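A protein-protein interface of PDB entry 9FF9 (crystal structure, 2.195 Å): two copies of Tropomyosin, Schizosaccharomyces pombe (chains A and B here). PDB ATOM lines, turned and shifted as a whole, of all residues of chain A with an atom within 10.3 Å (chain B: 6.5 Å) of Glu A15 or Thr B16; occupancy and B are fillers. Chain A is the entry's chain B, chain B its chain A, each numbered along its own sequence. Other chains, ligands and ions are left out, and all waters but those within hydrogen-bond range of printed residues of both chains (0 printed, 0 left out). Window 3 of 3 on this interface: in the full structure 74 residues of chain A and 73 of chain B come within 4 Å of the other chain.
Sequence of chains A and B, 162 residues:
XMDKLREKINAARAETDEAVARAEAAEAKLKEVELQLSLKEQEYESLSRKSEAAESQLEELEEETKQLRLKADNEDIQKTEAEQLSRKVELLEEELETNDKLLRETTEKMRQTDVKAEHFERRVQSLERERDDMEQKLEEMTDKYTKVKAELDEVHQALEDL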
ATOM      1  N   GLU A   7     -18.265 -24.067  16.671  1.00  0.00           N
ATOM      2  CA  GLU A   7     -16.971 -23.400  16.578  1.00  0.00           C
ATOM      3  C   GLU A   7     -16.048 -23.830  17.712  1.00  0.00           C
ATOM      4  O   GLU A   7     -14.915 -24.269  17.474  1.00  0.00           O
ATOM      5  CB  GLU A   7     -17.167 -21.883  16.586  1.00  0.00           C
ATOM      6  CG  GLU A   7     -15.899 -21.087  16.857  1.00  0.00           C
ATOM      7  CD  GLU A   7     -16.175 -19.609  17.058  1.00  0.00           C
ATOM      8  OE1 GLU A   7     -17.238 -19.137  16.603  1.00  0.00           O
ATOM      9  OE2 GLU A   7     -15.333 -18.921  17.675  1.00  0.00           O
ATOM     10  N   LYS A   8     -16.526 -23.722  18.955  1.00  0.00           N
ATOM     11  CA  LYS A   8     -15.698 -24.065  20.107  1.00  0.00           C
ATOM     12  C   LYS A   8     -15.326 -25.542  20.105  1.00  0.00           C
ATOM     13  O   LYS A   8     -14.169 -25.898  20.369  1.00  0.00           O
ATOM     14  CB  LYS A   8     -16.423 -23.700  21.403  1.00  0.00           C
ATOM     15  CG  LYS A   8     -16.632 -22.210  21.607  1.00  0.00           C
ATOM     16  CD  LYS A   8     -15.307 -21.479  21.726  1.00  0.00           C
ATOM     17  CE  LYS A   8     -15.516 -19.987  21.913  1.00  0.00           C
ATOM     18  NZ  LYS A   8     -16.262 -19.684  23.166  1.00  0.00           N
ATOM     19  N   ILE A   9     -16.291 -26.417  19.813  1.00  0.00           N
ATOM     20  CA  ILE A   9     -16.023 -27.854  19.832  1.00  0.00           C
ATOM     21  C   ILE A   9     -14.959 -28.208  18.802  1.00  0.00           C
ATOM     22  O   ILE A   9     -13.983 -28.908  19.105  1.00  0.00           O
ATOM     23  CB  ILE A   9     -17.322 -28.646  19.599  1.00  0.00           C
ATOM     24  CG1 ILE A   9     -18.279 -28.470  20.781  1.00  0.00           C
ATOM     25  CG2 ILE A   9     -17.017 -30.118  19.369  1.00  0.00           C
ATOM     26  CD1 ILE A   9     -17.694 -28.883  22.111  1.00  0.00           C
ATOM     27  N   ASN A  10     -15.130 -27.723  17.569  1.00  0.00           N
ATOM     28  CA  ASN A  10     -14.175 -28.033  16.512  1.00  0.00           C
ATOM     29  C   ASN A  10     -12.802 -27.458  16.823  1.00  0.00           C
ATOM     30  O   ASN A  10     -11.782 -28.121  16.597  1.00  0.00           O
ATOM     31  CB  ASN A  10     -14.688 -27.507  15.171  1.00  0.00           C
ATOM     32  CG  ASN A  10     -15.960 -28.199  14.723  1.00  0.00           C
ATOM     33  OD1 ASN A  10     -16.207 -29.353  15.070  1.00  0.00           O
ATOM     34  ND2 ASN A  10     -16.773 -27.495  13.945  1.00  0.00           N
ATOM     35  N   ALA A  11     -12.750 -26.230  17.347  1.00  0.00           N
ATOM     36  CA  ALA A  11     -11.464 -25.619  17.664  1.00  0.00           C
ATOM     37  C   ALA A  11     -10.726 -26.423  18.726  1.00  0.00           C
ATOM     38  O   ALA A  11      -9.543 -26.746  18.566  1.00  0.00           O
ATOM     39  CB  ALA A  11     -11.662 -24.175  18.122  1.00  0.00           C
ATOM     40  N   ALA A  12     -11.418 -26.767  19.816  1.00  0.00           N
ATOM     41  CA  ALA A  12     -10.787 -27.555  20.869  1.00  0.00           C
ATOM     42  C   ALA A  12     -10.325 -28.909  20.349  1.00  0.00           C
ATOM     43  O   ALA A  12      -9.199 -29.341  20.632  1.00  0.00           O
ATOM     44  CB  ALA A  12     -11.749 -27.738  22.040  1.00  0.00           C
ATOM     45  N   ARG A  13     -11.178 -29.596  19.584  1.00  0.00           N
ATOM     46  CA  ARG A  13     -10.831 -30.929  19.104  1.00  0.00           C
ATOM     47  C   ARG A  13      -9.624 -30.886  18.174  1.00  0.00           C
ATOM     48  O   ARG A  13      -8.686 -31.678  18.321  1.00  0.00           O
ATOM     49  CB  ARG A  13     -12.032 -31.561  18.401  1.00  0.00           C
ATOM     50  CG  ARG A  13     -11.734 -32.921  17.803  1.00  0.00           C
ATOM     51  CD  ARG A  13     -12.875 -33.410  16.932  1.00  0.00           C
ATOM     52  NE  ARG A  13     -12.460 -34.522  16.085  1.00  0.00           N
ATOM     53  CZ  ARG A  13     -11.865 -34.383  14.908  1.00  0.00           C
ATOM     54  NH1 ARG A  13     -11.598 -33.189  14.404  1.00  0.00           N
ATOM     55  NH2 ARG A  13     -11.526 -35.470  14.222  1.00  0.00           N
ATOM     56  N   ALA A  14      -9.630 -29.962  17.208  1.00  0.00           N
ATOM     57  CA  ALA A  14      -8.508 -29.853  16.281  1.00  0.00           C
ATOM     58  C   ALA A  14      -7.224 -29.475  17.007  1.00  0.00           C
ATOM     59  O   ALA A  14      -6.154 -30.027  16.715  1.00  0.00           O
ATOM     60  CB  ALA A  14      -8.827 -28.833  15.188  1.00  0.00           C
ATOM     61  N   GLU A  15      -7.306 -28.538  17.955  1.00  0.00           N
ATOM     62  CA  GLU A  15      -6.119 -28.126  18.697  1.00  0.00           C
ATOM     63  C   GLU A  15      -5.528 -29.296  19.473  1.00  0.00           C
ATOM     64  O   GLU A  15      -4.319 -29.560  19.400  1.00  0.00           O
ATOM     65  CB  GLU A  15      -6.479 -26.973  19.633  1.00  0.00           C
ATOM     66  CG  GLU A  15      -5.296 -26.305  20.309  1.00  0.00           C
ATOM     67  CD  GLU A  15      -5.724 -25.190  21.244  1.00  0.00           C
ATOM     68  OE1 GLU A  15      -6.936 -25.083  21.528  1.00  0.00           O
ATOM     69  OE2 GLU A  15      -4.850 -24.419  21.694  1.00  0.00           O
ATOM     70  N   THR A  16      -6.373 -30.017  20.217  1.00  0.00           N
ATOM     71  CA  THR A  16      -5.895 -31.168  20.976  1.00  0.00           C
ATOM     72  C   THR A  16      -5.298 -32.228  20.060  1.00  0.00           C
ATOM     73  O   THR A  16      -4.242 -32.796  20.365  1.00  0.00           O
ATOM     74  CB  THR A  16      -7.035 -31.765  21.803  1.00  0.00           C
ATOM     75  OG1 THR A  16      -7.578 -30.764  22.672  1.00  0.00           O
ATOM     76  CG2 THR A  16      -6.533 -32.934  22.637  1.00  0.00           C
ATOM     77  N   ASP A  17      -5.957 -32.508  18.932  1.00  0.00           N
ATOM     78  CA  ASP A  17      -5.470 -33.551  18.036  1.00  0.00           C
ATOM     79  C   ASP A  17      -4.118 -33.182  17.442  1.00  0.00           C
ATOM     80  O   ASP A  17      -3.203 -34.013  17.402  1.00  0.00           O
ATOM     81  CB  ASP A  17      -6.492 -33.813  16.933  1.00  0.00           C
ATOM     82  CG  ASP A  17      -7.773 -34.423  17.462  1.00  0.00           C
ATOM     83  OD1 ASP A  17      -7.710 -35.142  18.481  1.00  0.00           O
ATOM     84  OD2 ASP A  17      -8.841 -34.182  16.864  1.00  0.00           O
ATOM     85  N   GLU A  18      -3.966 -31.938  16.986  1.00  0.00           N
ATOM     86  CA  GLU A  18      -2.691 -31.520  16.414  1.00  0.00           C
ATOM     87  C   GLU A  18      -1.586 -31.540  17.465  1.00  0.00           C
ATOM     88  O   GLU A  18      -0.457 -31.969  17.185  1.00  0.00           O
ATOM     89  CB  GLU A  18      -2.830 -30.131  15.799  1.00  0.00           C
ATOM     90  CG  GLU A  18      -1.829 -29.831  14.701  1.00  0.00           C
ATOM     91  CD  GLU A  18      -2.066 -28.475  14.066  1.00  0.00           C
ATOM     92  OE1 GLU A  18      -2.561 -27.567  14.767  1.00  0.00           O
ATOM     93  OE2 GLU A  18      -1.767 -28.318  12.863  1.00  0.00           O
ATOM     94  N   ALA A  19      -1.897 -31.097  18.687  1.00  0.00           N
ATOM     95  CA  ALA A  19      -0.897 -31.103  19.749  1.00  0.00           C
ATOM     96  C   ALA A  19      -0.449 -32.523  20.081  1.00  0.00           C
ATOM     97  O   ALA A  19       0.754 -32.799  20.185  1.00  0.00           O
ATOM     98  CB  ALA A  19      -1.454 -30.407  20.991  1.00  0.00           C
ATOM     99  N   VAL A  20      -1.403 -33.445  20.245  1.00  0.00           N
ATOM    100  CA  VAL A  20      -1.025 -34.808  20.610  1.00  0.00           C
ATOM    101  C   VAL A  20      -0.318 -35.501  19.452  1.00  0.00           C
ATOM    102  O   VAL A  20       0.565 -36.337  19.674  1.00  0.00           O
ATOM    103  CB  VAL A  20      -2.243 -35.618  21.099  1.00  0.00           C
ATOM    104  CG1 VAL A  20      -2.892 -34.937  22.297  1.00  0.00           C
ATOM    105  CG2 VAL A  20      -3.250 -35.836  19.981  1.00  0.00           C
ATOM    106  N   ALA A  21      -0.660 -35.157  18.206  1.00  0.00           N
ATOM    107  CA  ALA A  21       0.050 -35.741  17.073  1.00  0.00           C
ATOM    108  C   ALA A  21       1.499 -35.277  17.034  1.00  0.00           C
ATOM    109  O   ALA A  21       2.411 -36.086  16.814  1.00  0.00           O
ATOM    110  CB  ALA A  21      -0.664 -35.391  15.767  1.00  0.00           C
ATOM    111  N   ARG A  22       1.731 -33.977  17.245  1.00  0.00           N
ATOM    112  CA  ARG A  22       3.103 -33.484  17.318  1.00  0.00           C
ATOM    113  C   ARG A  22       3.865 -34.158  18.452  1.00  0.00           C
ATOM    114  O   ARG A  22       5.025 -34.560  18.283  1.00  0.00           O
ATOM    115  CB  ARG A  22       3.106 -31.965  17.489  1.00  0.00           C
ATOM    116  CG  ARG A  22       4.471 -31.324  17.295  1.00  0.00           C
ATOM    117  CD  ARG A  22       4.356 -29.815  17.148  1.00  0.00           C
ATOM    118  NE  ARG A  22       4.319 -29.125  18.431  1.00  0.00           N
ATOM    119  CZ  ARG A  22       5.368 -28.550  19.003  1.00  0.00           C
ATOM    120  NH1 ARG A  22       6.565 -28.576  18.439  1.00  0.00           N
ATOM    121  NH2 ARG A  22       5.213 -27.931  20.170  1.00  0.00           N
ATOM    122  N   ALA A  23       3.220 -34.306  19.613  1.00  0.00           N
ATOM    123  CA  ALA A  23       3.875 -34.952  20.747  1.00  0.00           C
ATOM    124  C   ALA A  23       4.239 -36.400  20.435  1.00  0.00           C
ATOM    125  O   ALA A  23       5.342 -36.853  20.759  1.00  0.00           O
ATOM    126  CB  ALA A  23       2.976 -34.879  21.981  1.00  0.00           C
ATOM    127  N   ALA B  11     -10.804 -29.701  30.028  1.00  0.00           N
ATOM    128  CA  ALA B  11     -10.000 -30.915  29.946  1.00  0.00           C
ATOM    129  C   ALA B  11      -9.255 -31.001  28.621  1.00  0.00           C
ATOM    130  O   ALA B  11      -8.146 -31.546  28.567  1.00  0.00           O
ATOM    131  CB  ALA B  11     -10.885 -32.143  30.143  1.00  0.00           C
ATOM    132  N   ALA B  12      -9.841 -30.470  27.546  1.00  0.00           N
ATOM    133  CA  ALA B  12      -9.161 -30.477  26.256  1.00  0.00           C
ATOM    134  C   ALA B  12      -8.027 -29.462  26.227  1.00  0.00           C
ATOM    135  O   ALA B  12      -6.962 -29.729  25.658  1.00  0.00           O
ATOM    136  CB  ALA B  12     -10.160 -30.201  25.133  1.00  0.00           C
ATOM    137  N   ARG B  13      -8.234 -28.292  26.834  1.00  0.00           N
ATOM    138  CA  ARG B  13      -7.170 -27.295  26.876  1.00  0.00           C
ATOM    139  C   ARG B  13      -6.021 -27.755  27.765  1.00  0.00           C
ATOM    140  O   ARG B  13      -4.851 -27.507  27.451  1.00  0.00           O
ATOM    141  CB  ARG B  13      -7.723 -25.950  27.347  1.00  0.00           C
ATOM    142  CG  ARG B  13      -8.738 -25.327  26.395  1.00  0.00           C
ATOM    143  CD  ARG B  13      -8.805 -23.807  26.555  1.00  0.00           C
ATOM    144  NE  ARG B  13      -9.672 -23.183  25.559  1.00  0.00           N
ATOM    145  CZ  ARG B  13     -10.907 -22.764  25.800  1.00  0.00           C
ATOM    146  NH1 ARG B  13     -11.451 -22.872  27.002  1.00  0.00           N
ATOM    147  NH2 ARG B  13     -11.612 -22.216  24.812  1.00  0.00           N
ATOM    148  N   ALA B  14      -6.332 -28.432  28.873  1.00  0.00           N
ATOM    149  CA  ALA B  14      -5.276 -29.015  29.694  1.00  0.00           C
ATOM    150  C   ALA B  14      -4.569 -30.147  28.957  1.00  0.00           C
ATOM    151  O   ALA B  14      -3.354 -30.324  29.100  1.00  0.00           O
ATOM    152  CB  ALA B  14      -5.853 -29.515  31.019  1.00  0.00           C
ATOM    153  N   GLU B  15      -5.315 -30.922  28.167  1.00  0.00           N
ATOM    154  CA  GLU B  15      -4.695 -31.978  27.375  1.00  0.00           C
ATOM    155  C   GLU B  15      -3.810 -31.406  26.277  1.00  0.00           C
ATOM    156  O   GLU B  15      -2.802 -32.019  25.906  1.00  0.00           O
ATOM    157  CB  GLU B  15      -5.770 -32.886  26.777  1.00  0.00           C
ATOM    158  CG  GLU B  15      -5.219 -34.088  26.029  1.00  0.00           C
ATOM    159  CD  GLU B  15      -6.303 -35.036  25.582  1.00  0.00           C
ATOM    160  OE1 GLU B  15      -7.483 -34.780  25.895  1.00  0.00           O
ATOM    161  OE2 GLU B  15      -5.976 -36.039  24.919  1.00  0.00           O
ATOM    162  N   THR B  16      -4.169 -30.241  25.738  1.00  0.00           N
ATOM    163  CA  THR B  16      -3.310 -29.595  24.754  1.00  0.00           C
ATOM    164  C   THR B  16      -2.074 -29.000  25.415  1.00  0.00           C
ATOM    165  O   THR B  16      -0.972 -29.060  24.856  1.00  0.00           O
ATOM    166  CB  THR B  16      -4.094 -28.521  24.001  1.00  0.00           C
ATOM    167  OG1 THR B  16      -5.223 -29.122  23.356  1.00  0.00           O
ATOM    168  CG2 THR B  16      -3.217 -27.851  22.954  1.00  0.00           C
ATOM    169  N   ASP B  17      -2.235 -28.433  26.613  1.00  0.00           N
ATOM    170  CA  ASP B  17      -1.104 -27.818  27.299  1.00  0.00           C
ATOM    171  C   ASP B  17      -0.078 -28.854  27.739  1.00  0.00           C
ATOM    172  O   ASP B  17       1.126 -28.573  27.730  1.00  0.00           O
ATOM    173  CB  ASP B  17      -1.600 -27.006  28.495  1.00  0.00           C
ATOM    174  CG  ASP B  17      -2.364 -25.763  28.077  1.00  0.00           C
ATOM    175  OD1 ASP B  17      -2.011 -25.171  27.034  1.00  0.00           O
ATOM    176  OD2 ASP B  17      -3.318 -25.377  28.786  1.00  0.00           O
ATOM    177  N   GLU B  18      -0.523 -30.050  28.131  1.00  0.00           N
ATOM    178  CA  GLU B  18       0.433 -31.101  28.463  1.00  0.00           C
ATOM    179  C   GLU B  18       1.081 -31.669  27.210  1.00  0.00           C
ATOM    180  O   GLU B  18       2.219 -32.147  27.266  1.00  0.00           O
ATOM    181  CB  GLU B  18      -0.246 -32.214  29.268  1.00  0.00           C
ATOM    182  CG  GLU B  18      -1.410 -32.910  28.567  1.00  0.00           C
ATOM    183  CD  GLU B  18      -0.973 -34.042  27.650  1.00  0.00           C
ATOM    184  OE1 GLU B  18       0.184 -34.496  27.772  1.00  0.00           O
ATOM    185  OE2 GLU B  18      -1.788 -34.478  26.808  1.00  0.00           O
ATOM    186  N   ALA B  19       0.378 -31.623  26.078  1.00  0.00           N
ATOM    187  CA  ALA B  19       0.936 -32.151  24.839  1.00  0.00           C
ATOM    188  C   ALA B  19       2.013 -31.235  24.273  1.00  0.00           C
ATOM    189  O   ALA B  19       3.025 -31.715  23.752  1.00  0.00           O
ATOM    190  CB  ALA B  19      -0.174 -32.371  23.814  1.00  0.00           C
ATOM    191  N   VAL B  20       1.819 -29.915  24.361  1.00  0.00           N
ATOM    192  CA  VAL B  20       2.837 -28.999  23.854  1.00  0.00           C
ATOM    193  C   VAL B  20       4.059 -28.994  24.764  1.00  0.00           C
ATOM    194  O   VAL B  20       5.189 -28.829  24.291  1.00  0.00           O
ATOM    195  CB  VAL B  20       2.259 -27.581  23.667  1.00  0.00           C
ATOM    196  CG1 VAL B  20       1.152 -27.594  22.624  1.00  0.00           C
ATOM    197  CG2 VAL B  20       1.758 -27.011  24.989  1.00  0.00           C
ATOM    198  N   ALA B  21       3.865 -29.178  26.072  1.00  0.00           N
ATOM    199  CA  ALA B  21       5.011 -29.330  26.961  1.00  0.00           C
ATOM    200  C   ALA B  21       5.665 -30.693  26.787  1.00  0.00           C
ATOM    201  O   ALA B  21       6.884 -30.821  26.952  1.00  0.00           O
ATOM    202  CB  ALA B  21       4.587 -29.119  28.413  1.00  0.00           C
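The backbone carbonyl oxygen of Ala B12 lies within hydrogen-bond range of the side-chain hydroxyl of Thr A16 (3.2 Å). The side-chain hydroxyl (OG1) of Thr B16 lies within hydrogen-bond range of the side-chain hydroxyl (OG1) of Thr A16 (3.0 Å).
OG1 of Thr B16 sits at hydrogen-bond distance from O of Ala B12. The backbone carbonyl oxygen of Ala A12 lies within hydrogen-bond range of the side-chain hydroxyl of Thr A16.
Among the printed residues, pairs that only touch across the chains: Thr A16 with Glu B15 (3.6 Å), Ala A23 with Ala B19 (3.6 Å), Ala A19 with Ala B19 (3.7 Å), Ala A19 with Thr B16 (3.7 Å), Glu A15 with Thr B16 (3.7 Å) and Val A20 with Ala B19 (3.9 Å).
Of the printed residues of chain B, Thr A16 touches Ala B12 (3.2 Å), Glu B15 (3.6 Å) and Thr B16 (3.0 Å). Printed residues of chain B within 4 Å of Ala A19: Thr B16 (3.7 Å) and Ala B19 (3.7 Å). Of the printed residues of chain B, Val A20 touches Ala B19 (3.9 Å). Of the printed residues of chain B, Ala A23 touches Ala B19. Ala B12 touches one residue of chain A. Of chain A, only Thr A16 comes within 4 Å of Glu B15. Of chain A, only Glu A15, Thr A16 and Ala A19 come within 4 Å of Thr B16. No residue of chain A comes within 4 Å of Val B20. The nearest printed residue of chain B that does not touch Ala A19 is Val B20 (4.2 Å).
Of the 11 printed residues of chain B, 4 touch a printed residue of chain A. Hydrophobic or aromatic side chains of chain B within 4 Å of the printed part of chain A: Ala B12 and Ala B19. Hydrophobic or aromatic side chains of chain A within 4 Å of the printed part of chain B: Ala A19 and Ala A23. Among the printed residues, 8 pairs touch across the chains. Among the printed residues, no Asp or Glu carboxylate lies within 4 Å of a Lys or Arg side-chain nitrogen of the other chain.
Glu A15 touches Thr B16, and with the chains exchanged Thr A16 touches Glu B15. Thr A16 touches Ala B12, but with the chains exchanged Ala A12 does not touch Thr B16 (4.8 Å). Thr A16 touches its own counterpart, Thr B16. Ala A19 touches its own counterpart, Ala B19.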
